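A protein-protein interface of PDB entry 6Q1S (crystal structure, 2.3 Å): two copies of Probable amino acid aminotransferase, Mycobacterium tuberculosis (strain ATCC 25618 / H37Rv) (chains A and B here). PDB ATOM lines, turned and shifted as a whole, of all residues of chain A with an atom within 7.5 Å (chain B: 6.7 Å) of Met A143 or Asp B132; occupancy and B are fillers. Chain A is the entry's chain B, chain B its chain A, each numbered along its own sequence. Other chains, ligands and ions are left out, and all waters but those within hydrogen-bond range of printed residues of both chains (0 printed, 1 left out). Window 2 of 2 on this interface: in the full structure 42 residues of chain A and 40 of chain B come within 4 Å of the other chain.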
ATOM      1  N   GLY A 134     -37.007 -19.954  31.511  1.00  0.00           N
ATOM      2  CA  GLY A 134     -35.930 -19.019  31.721  1.00  0.00           C
ATOM      3  C   GLY A 134     -35.139 -18.684  30.481  1.00  0.00           C
ATOM      4  O   GLY A 134     -34.333 -17.748  30.514  1.00  0.00           O
ATOM      5  N   LEU A 135     -35.375 -19.388  29.379  1.00  0.00           N
ATOM      6  CA  LEU A 135     -34.676 -19.114  28.138  1.00  0.00           C
ATOM      7  C   LEU A 135     -35.561 -18.312  27.203  1.00  0.00           C
ATOM      8  O   LEU A 135     -36.763 -18.572  27.113  1.00  0.00           O
ATOM      9  CB  LEU A 135     -34.287 -20.417  27.436  1.00  0.00           C
ATOM     10  CG  LEU A 135     -33.087 -21.234  27.906  1.00  0.00           C
ATOM     11  CD1 LEU A 135     -33.052 -22.565  27.172  1.00  0.00           C
ATOM     12  CD2 LEU A 135     -31.813 -20.457  27.642  1.00  0.00           C
ATOM     13  N   PRO A 136     -34.992 -17.329  26.521  1.00  0.00           N
ATOM     14  CA  PRO A 136     -35.714 -16.659  25.440  1.00  0.00           C
ATOM     15  C   PRO A 136     -35.631 -17.461  24.149  1.00  0.00           C
ATOM     16  O   PRO A 136     -34.778 -18.333  23.972  1.00  0.00           O
ATOM     17  CB  PRO A 136     -34.999 -15.310  25.316  1.00  0.00           C
ATOM     18  CG  PRO A 136     -33.623 -15.581  25.800  1.00  0.00           C
ATOM     19  CD  PRO A 136     -33.718 -16.662  26.837  1.00  0.00           C
ATOM     20  N   ASP A 138     -34.600 -16.743  21.299  1.00  0.00           N
ATOM     21  CA  ASP A 138     -33.368 -16.580  20.536  1.00  0.00           C
ATOM     22  C   ASP A 138     -32.232 -17.481  21.006  1.00  0.00           C
ATOM     23  O   ASP A 138     -31.172 -17.491  20.370  1.00  0.00           O
ATOM     24  CB  ASP A 138     -32.894 -15.123  20.628  1.00  0.00           C
ATOM     25  CG  ASP A 138     -32.657 -14.669  22.069  1.00  0.00           C
ATOM     26  OD1 ASP A 138     -32.487 -15.529  22.961  1.00  0.00           O
ATOM     27  OD2 ASP A 138     -32.637 -13.444  22.315  1.00  0.00           O
ATOM     28  N   GLY A 139     -32.429 -18.250  22.077  1.00  0.00           N
ATOM     29  CA  GLY A 139     -31.309 -18.917  22.722  1.00  0.00           C
ATOM     30  C   GLY A 139     -30.649 -20.027  21.929  1.00  0.00           C
ATOM     31  O   GLY A 139     -29.467 -20.317  22.139  1.00  0.00           O
ATOM     32  N   GLY A 140     -31.380 -20.665  21.015  1.00  0.00           N
ATOM     33  CA  GLY A 140     -30.811 -21.815  20.327  1.00  0.00           C
ATOM     34  C   GLY A 140     -29.700 -21.454  19.358  1.00  0.00           C
ATOM     35  O   GLY A 140     -28.629 -22.068  19.366  1.00  0.00           O
ATOM     36  N   ASP A 141     -29.930 -20.448  18.519  1.00  0.00           N
ATOM     37  CA  ASP A 141     -28.953 -20.057  17.510  1.00  0.00           C
ATOM     38  C   ASP A 141     -28.071 -18.887  17.930  1.00  0.00           C
ATOM     39  O   ASP A 141     -26.883 -18.868  17.595  1.00  0.00           O
ATOM     40  CB  ASP A 141     -29.667 -19.737  16.195  1.00  0.00           C
ATOM     41  CG  ASP A 141     -30.259 -20.975  15.548  1.00  0.00           C
ATOM     42  OD1 ASP A 141     -29.659 -21.498  14.585  1.00  0.00           O
ATOM     43  OD2 ASP A 141     -31.305 -21.451  16.035  1.00  0.00           O
ATOM     44  N   ALA A 142     -28.616 -17.911  18.660  1.00  0.00           N
ATOM     45  CA  ALA A 142     -27.812 -16.762  19.063  1.00  0.00           C
ATOM     46  C   ALA A 142     -26.816 -17.119  20.157  1.00  0.00           C
ATOM     47  O   ALA A 142     -25.789 -16.444  20.289  1.00  0.00           O
ATOM     48  CB  ALA A 142     -28.713 -15.622  19.537  1.00  0.00           C
ATOM     49  N   MET A 143     -27.089 -18.167  20.930  1.00  0.00           N
ATOM     50  CA  MET A 143     -26.225 -18.605  22.024  1.00  0.00           C
ATOM     51  C   MET A 143     -25.942 -20.085  21.814  1.00  0.00           C
ATOM     52  O   MET A 143     -26.521 -20.949  22.487  1.00  0.00           O
ATOM     53  CB  MET A 143     -26.868 -18.315  23.382  1.00  0.00           C
ATOM     54  CG  MET A 143     -27.451 -16.905  23.478  1.00  0.00           C
ATOM     55  SD  MET A 143     -28.213 -16.445  25.049  1.00  0.00           S
ATOM     56  CE  MET A 143     -29.219 -17.877  25.389  1.00  0.00           C
ATOM     57  N   PRO A 144     -25.043 -20.414  20.879  1.00  0.00           N
ATOM     58  CA  PRO A 144     -24.740 -21.828  20.614  1.00  0.00           C
ATOM     59  C   PRO A 144     -23.978 -22.505  21.734  1.00  0.00           C
ATOM     60  O   PRO A 144     -24.010 -23.739  21.821  1.00  0.00           O
ATOM     61  CB  PRO A 144     -23.907 -21.773  19.328  1.00  0.00           C
ATOM     62  CG  PRO A 144     -23.265 -20.426  19.364  1.00  0.00           C
ATOM     63  CD  PRO A 144     -24.269 -19.509  20.012  1.00  0.00           C
ATOM     64  N   TRP A 145     -23.301 -21.744  22.598  1.00  0.00           N
ATOM     65  CA  TRP A 145     -22.541 -22.355  23.681  1.00  0.00           C
ATOM     66  C   TRP A 145     -23.438 -23.074  24.677  1.00  0.00           C
ATOM     67  O   TRP A 145     -22.952 -23.928  25.425  1.00  0.00           O
ATOM     68  CB  TRP A 145     -21.715 -21.294  24.407  1.00  0.00           C
ATOM     69  CG  TRP A 145     -22.500 -20.060  24.734  1.00  0.00           C
ATOM     70  CD1 TRP A 145     -23.260 -19.841  25.848  1.00  0.00           C
ATOM     71  CD2 TRP A 145     -22.603 -18.873  23.940  1.00  0.00           C
ATOM     72  NE1 TRP A 145     -23.832 -18.593  25.792  1.00  0.00           N
ATOM     73  CE2 TRP A 145     -23.444 -17.979  24.631  1.00  0.00           C
ATOM     74  CE3 TRP A 145     -22.066 -18.482  22.711  1.00  0.00           C
ATOM     75  CZ2 TRP A 145     -23.759 -16.718  24.136  1.00  0.00           C
ATOM     76  CZ3 TRP A 145     -22.381 -17.229  22.219  1.00  0.00           C
ATOM     77  CH2 TRP A 145     -23.220 -16.362  22.930  1.00  0.00           C
ATOM     78  N   LEU A 146     -24.730 -22.745  24.711  1.00  0.00           N
ATOM     79  CA  LEU A 146     -25.663 -23.453  25.577  1.00  0.00           C
ATOM     80  C   LEU A 146     -26.139 -24.773  24.989  1.00  0.00           C
ATOM     81  O   LEU A 146     -26.852 -25.508  25.681  1.00  0.00           O
ATOM     82  CB  LEU A 146     -26.869 -22.570  25.900  1.00  0.00           C
ATOM     83  CG  LEU A 146     -26.564 -21.267  26.639  1.00  0.00           C
ATOM     84  CD1 LEU A 146     -27.860 -20.598  27.043  1.00  0.00           C
ATOM     85  CD2 LEU A 146     -25.696 -21.520  27.859  1.00  0.00           C
ATOM     86  N   ILE A 147     -25.769 -25.077  23.738  1.00  0.00           N
ATOM     87  CA  ILE A 147     -26.033 -26.343  23.048  1.00  0.00           C
ATOM     88  C   ILE A 147     -27.427 -26.883  23.353  1.00  0.00           C
ATOM     89  O   ILE A 147     -27.604 -28.083  23.590  1.00  0.00           O
ATOM     90  CB  ILE A 147     -24.948 -27.398  23.366  1.00  0.00           C
ATOM     91  CG1 ILE A 147     -24.827 -27.675  24.869  1.00  0.00           C
ATOM     92  CG2 ILE A 147     -23.602 -26.957  22.808  1.00  0.00           C
ATOM     93  CD1 ILE A 147     -24.515 -29.103  25.211  1.00  0.00           C
ATOM     94  N   ALA A 148     -28.432 -26.002  23.326  1.00  0.00           N
ATOM     95  CA  ALA A 148     -29.788 -26.401  23.683  1.00  0.00           C
ATOM     96  C   ALA A 148     -30.395 -27.401  22.707  1.00  0.00           C
ATOM     97  O   ALA A 148     -31.383 -28.057  23.051  1.00  0.00           O
ATOM     98  CB  ALA A 148     -30.689 -25.170  23.780  1.00  0.00           C
ATOM     99  N   SER A 149     -29.834 -27.540  21.509  1.00  0.00           N
ATOM    100  CA  SER A 149     -30.332 -28.506  20.539  1.00  0.00           C
ATOM    101  C   SER A 149     -29.655 -29.864  20.653  1.00  0.00           C
ATOM    102  O   SER A 149     -29.988 -30.770  19.883  1.00  0.00           O
ATOM    103  CB  SER A 149     -30.162 -27.967  19.115  1.00  0.00           C
ATOM    104  OG  SER A 149     -28.792 -27.827  18.785  1.00  0.00           O
ATOM    105  N   PRO A 213     -34.505 -22.581  21.281  1.00  0.00           N
ATOM    106  CA  PRO A 213     -33.574 -23.402  22.070  1.00  0.00           C
ATOM    107  C   PRO A 213     -34.187 -24.718  22.525  1.00  0.00           C
ATOM    108  O   PRO A 213     -34.338 -24.945  23.729  1.00  0.00           O
ATOM    109  CB  PRO A 213     -33.240 -22.500  23.264  1.00  0.00           C
ATOM    110  CG  PRO A 213     -34.432 -21.609  23.397  1.00  0.00           C
ATOM    111  CD  PRO A 213     -34.897 -21.352  21.995  1.00  0.00           C
ATOM    112  N   THR B 130     -17.020 -12.832  28.814  1.00  0.00           N
ATOM    113  CA  THR B 130     -18.384 -12.871  29.312  1.00  0.00           C
ATOM    114  C   THR B 130     -19.280 -13.561  28.295  1.00  0.00           C
ATOM    115  O   THR B 130     -19.164 -13.334  27.088  1.00  0.00           O
ATOM    116  CB  THR B 130     -18.897 -11.459  29.591  1.00  0.00           C
ATOM    117  OG1 THR B 130     -18.829 -10.681  28.390  1.00  0.00           O
ATOM    118  CG2 THR B 130     -18.057 -10.791  30.669  1.00  0.00           C
ATOM    119  N   LEU B 131     -20.172 -14.414  28.785  1.00  0.00           N
ATOM    120  CA  LEU B 131     -21.085 -15.148  27.924  1.00  0.00           C
ATOM    121  C   LEU B 131     -22.460 -15.169  28.567  1.00  0.00           C
ATOM    122  O   LEU B 131     -22.583 -15.306  29.787  1.00  0.00           O
ATOM    123  CB  LEU B 131     -20.600 -16.578  27.661  1.00  0.00           C
ATOM    124  CG  LEU B 131     -19.462 -16.731  26.648  1.00  0.00           C
ATOM    125  CD1 LEU B 131     -18.961 -18.167  26.622  1.00  0.00           C
ATOM    126  CD2 LEU B 131     -19.907 -16.292  25.263  1.00  0.00           C
ATOM    127  N   ASP B 132     -23.489 -15.021  27.739  1.00  0.00           N
ATOM    128  CA  ASP B 132     -24.853 -15.066  28.239  1.00  0.00           C
ATOM    129  C   ASP B 132     -25.156 -16.462  28.772  1.00  0.00           C
ATOM    130  O   ASP B 132     -24.929 -17.464  28.088  1.00  0.00           O
ATOM    131  CB  ASP B 132     -25.833 -14.676  27.133  1.00  0.00           C
ATOM    132  CG  ASP B 132     -27.186 -14.258  27.673  1.00  0.00           C
ATOM    133  OD1 ASP B 132     -27.657 -14.874  28.651  1.00  0.00           O
ATOM    134  OD2 ASP B 132     -27.777 -13.306  27.118  1.00  0.00           O
ATOM    135  N   ARG B 133     -25.674 -16.517  30.000  1.00  0.00           N
ATOM    136  CA  ARG B 133     -26.008 -17.786  30.638  1.00  0.00           C
ATOM    137  C   ARG B 133     -27.324 -18.350  30.125  1.00  0.00           C
ATOM    138  O   ARG B 133     -27.528 -19.571  30.156  1.00  0.00           O
ATOM    139  CB  ARG B 133     -26.068 -17.590  32.157  1.00  0.00           C
ATOM    140  CG  ARG B 133     -26.592 -18.772  32.970  1.00  0.00           C
ATOM    141  CD  ARG B 133     -25.707 -20.005  32.839  1.00  0.00           C
ATOM    142  NE  ARG B 133     -26.197 -21.121  33.645  1.00  0.00           N
ATOM    143  CZ  ARG B 133     -27.060 -22.040  33.216  1.00  0.00           C
ATOM    144  NH1 ARG B 133     -27.533 -21.986  31.978  1.00  0.00           N
ATOM    145  NH2 ARG B 133     -27.446 -23.015  34.027  1.00  0.00           N
ATOM    146  N   GLY B 134     -28.219 -17.492  29.650  1.00  0.00           N
ATOM    147  CA  GLY B 134     -29.525 -17.915  29.211  1.00  0.00           C
ATOM    148  C   GLY B 134     -30.588 -17.853  30.280  1.00  0.00           C
ATOM    149  O   GLY B 134     -31.767 -18.059  29.971  1.00  0.00           O
ATOM    150  N   LEU B 135     -30.207 -17.603  31.529  1.00  0.00           N
ATOM    151  CA  LEU B 135     -31.097 -17.438  32.660  1.00  0.00           C
ATOM    152  C   LEU B 135     -31.175 -15.969  33.059  1.00  0.00           C
ATOM    153  O   LEU B 135     -30.162 -15.264  33.003  1.00  0.00           O
ATOM    154  CB  LEU B 135     -30.626 -18.258  33.865  1.00  0.00           C
ATOM    155  CG  LEU B 135     -30.897 -19.761  33.794  1.00  0.00           C
ATOM    156  CD1 LEU B 135     -30.251 -20.479  34.971  1.00  0.00           C
ATOM    157  CD2 LEU B 135     -32.388 -20.033  33.739  1.00  0.00           C
ATOM    158  N   VAL B 161     -19.338 -24.779  27.375  1.00  0.00           N
ATOM    159  CA  VAL B 161     -19.063 -23.345  27.383  1.00  0.00           C
ATOM    160  C   VAL B 161     -17.566 -23.087  27.508  1.00  0.00           C
ATOM    161  O   VAL B 161     -17.016 -22.197  26.848  1.00  0.00           O
ATOM    162  CB  VAL B 161     -19.859 -22.660  28.511  1.00  0.00           C
ATOM    163  CG1 VAL B 161     -19.286 -21.289  28.823  1.00  0.00           C
ATOM    164  CG2 VAL B 161     -21.326 -22.546  28.130  1.00  0.00           C
ATOM    165  N   VAL B 173     -14.612 -18.426  31.620  1.00  0.00           N
ATOM    166  CA  VAL B 173     -15.835 -17.741  31.214  1.00  0.00           C
ATOM    167  C   VAL B 173     -16.467 -17.104  32.444  1.00  0.00           C
ATOM    168  O   VAL B 173     -16.392 -17.655  33.547  1.00  0.00           O
ATOM    169  CB  VAL B 173     -16.821 -18.713  30.525  1.00  0.00           C
ATOM    170  CG1 VAL B 173     -18.206 -18.093  30.373  1.00  0.00           C
ATOM    171  CG2 VAL B 173     -16.288 -19.144  29.173  1.00  0.00           C
ATOM    172  N   ILE B 174     -17.077 -15.935  32.264  1.00  0.00           N
ATOM    173  CA  ILE B 174     -17.900 -15.310  33.292  1.00  0.00           C
ATOM    174  C   ILE B 174     -19.329 -15.269  32.772  1.00  0.00           C
ATOM    175  O   ILE B 174     -19.621 -14.587  31.781  1.00  0.00           O
ATOM    176  CB  ILE B 174     -17.398 -13.908  33.660  1.00  0.00           C
ATOM    177  CG1 ILE B 174     -16.042 -14.005  34.362  1.00  0.00           C
ATOM    178  CG2 ILE B 174     -18.402 -13.203  34.559  1.00  0.00           C
ATOM    179  CD1 ILE B 174     -15.465 -12.669  34.772  1.00  0.00           C
ATOM    180  N   PHE B 175     -20.225 -15.994  33.438  1.00  0.00           N
ATOM    181  CA  PHE B 175     -21.619 -16.033  33.016  1.00  0.00           C
ATOM    182  C   PHE B 175     -22.308 -14.721  33.356  1.00  0.00           C
ATOM    183  O   PHE B 175     -22.177 -14.207  34.471  1.00  0.00           O
ATOM    184  CB  PHE B 175     -22.359 -17.182  33.699  1.00  0.00           C
ATOM    185  CG  PHE B 175     -22.245 -18.497  32.988  1.00  0.00           C
ATOM    186  CD1 PHE B 175     -22.475 -18.587  31.627  1.00  0.00           C
ATOM    187  CD2 PHE B 175     -21.938 -19.650  33.692  1.00  0.00           C
ATOM    188  CE1 PHE B 175     -22.380 -19.801  30.973  1.00  0.00           C
ATOM    189  CE2 PHE B 175     -21.842 -20.868  33.046  1.00  0.00           C
ATOM    190  CZ  PHE B 175     -22.064 -20.943  31.683  1.00  0.00           C
ATOM    191  N   VAL B 176     -23.040 -14.178  32.392  1.00  0.00           N
ATOM    192  CA  VAL B 176     -23.867 -12.999  32.596  1.00  0.00           C
ATOM    193  C   VAL B 176     -25.304 -13.382  32.280  1.00  0.00           C
ATOM    194  O   VAL B 176     -25.564 -14.138  31.336  1.00  0.00           O
ATOM    195  CB  VAL B 176     -23.403 -11.805  31.735  1.00  0.00           C
ATOM    196  CG1 VAL B 176     -22.012 -11.357  32.163  1.00  0.00           C
ATOM    197  CG2 VAL B 176     -23.414 -12.164  30.255  1.00  0.00           C
ATOM    198  N   SER B 177     -26.235 -12.889  33.089  1.00  0.00           N
ATOM    199  CA  SER B 177     -27.628 -13.203  32.844  1.00  0.00           C
ATOM    200  C   SER B 177     -28.119 -12.454  31.612  1.00  0.00           C
ATOM    201  O   SER B 177     -27.501 -11.491  31.150  1.00  0.00           O
ATOM    202  CB  SER B 177     -28.483 -12.842  34.058  1.00  0.00           C
ATOM    203  OG  SER B 177     -28.470 -11.445  34.297  1.00  0.00           O
ATOM    204  N   THR B 178     -29.250 -12.915  31.072  1.00  0.00           N
ATOM    205  CA  THR B 178     -29.858 -12.214  29.948  1.00  0.00           C
ATOM    206  C   THR B 178     -30.214 -10.791  30.341  1.00  0.00           C
ATOM    207  O   THR B 178     -30.220  -9.889  29.495  1.00  0.00           O
ATOM    208  CB  THR B 178     -31.104 -12.957  29.470  1.00  0.00           C
ATOM    209  OG1 THR B 178     -31.977 -13.180  30.582  1.00  0.00           O
ATOM    210  CG2 THR B 178     -30.728 -14.297  28.863  1.00  0.00           C
ATOM    211  N   ASP B 179     -30.502 -10.578  31.626  1.00  0.00           N
ATOM    212  CA  ASP B 179     -30.740  -9.248  32.165  1.00  0.00           C
ATOM    213  C   ASP B 179     -29.462  -8.420  32.232  1.00  0.00           C
ATOM    214  O   ASP B 179     -29.538  -7.197  32.381  1.00  0.00           O
ATOM    215  CB  ASP B 179     -31.366  -9.380  33.556  1.00  0.00           C
ATOM    216  CG  ASP B 179     -32.157  -8.160  33.962  1.00  0.00           C
ATOM    217  OD1 ASP B 179     -32.161  -7.164  33.210  1.00  0.00           O
ATOM    218  OD2 ASP B 179     -32.787  -8.204  35.042  1.00  0.00           O
ATOM    219  N   GLY B 180     -28.298  -9.053  32.135  1.00  0.00           N
ATOM    220  CA  GLY B 180     -27.034  -8.345  32.134  1.00  0.00           C
ATOM    221  C   GLY B 180     -26.282  -8.302  33.446  1.00  0.00           C
ATOM    222  O   GLY B 180     -25.334  -7.517  33.564  1.00  0.00           O
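Gly A134 touches Leu B135. Gly B134 touches Leu A135 (O to CD2, 3.3 Å). Gly B134 touches Pro A136. Met A143 touches Gly B134. Trp A145 touches Leu B131 (CD2 to CD2, 3.96 Å). Val B161 touches Trp A145. Arg B133 touches Leu A146. Leu A146 touches Gly B134.
Met A143 touches just these residues of chain B: Asp B132 (3.6 Å) and Gly B134 (3.8 Å). Asp B132 touches just these residues of chain A: Met A143 and Trp A145. Of the printed residues of chain B, Trp A145 touches Leu B131 (3.96 Å), Asp B132 (2.8 Å) and Val B161 (3.4 Å). Of the printed residues of chain A, Arg B133 touches Leu A146 (3.3 Å). Printed residues of chain A within 4 Å of Leu B131: Trp A145. Gly A139 touches none of the printed residues of chain B. The nearest residue of chain B that does not touch Met A143 is Thr B178 (5.0 Å).
Gly A134 touches its own counterpart, Gly B134. Gly A134 touches Leu B135, and with the chains exchanged Leu A135 touches Gly B134. 2 positions are printed for both chains. Of the 11 pairs that touch across the chains among the printed residues, 3 have their exchanged pair printed and touching as well.
O of Ile B174 lies within hydrogen-bond range of N of Leu B131. The backbone carbonyl oxygen (O) of Leu B131 lies within hydrogen-bond range of the backbone NH (N) of Val B176 (2.9 Å). N of Gly B134 is in hydrogen-bond range of OD1 of Asp B132 (2.9 Å). The side-chain carboxylate (OD1) of Asp B132 lies close to the backbone NH (N) of Thr B178 (3.5 Å). N of Arg B133 sits at hydrogen-bond distance from O of Val B176 (2.7 Å). The backbone NH (N) of Thr B178 lies within hydrogen-bond range of the backbone carbonyl oxygen (O) of Leu B135 (3.2 Å).
O of Asp B132 sits at hydrogen-bond distance from NE1 of Trp A145 (2.8 Å). The backbone carbonyl oxygen of Gly A134 sits close to the backbone carbonyl oxygen of Gly B134 (2.6 Å). SD of Met A143 sits close to OD2 of Asp B132 (3.8 Å).
Of the 16 printed residues of chain A, 6 touch a printed residue of chain B. Hydrophobic or aromatic side chains of chain A within 4 Å of the printed part of chain B: Leu A135, Pro A136, Met A143, Trp A145 and Leu A146. Printed residues of chain B that touch a printed residue of chain A: Leu B131, Asp B132, Arg B133, Gly B134, Leu B135 and Val B161. Hydrophobic or aromatic side chains of chain B within 4 Å of the printed part of chain A: Leu B131 and Val B161. Among the printed residues, no Asp or Glu carboxylate lies within 4 Å of a Lys or Arg side-chain nitrogen of the other chain.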
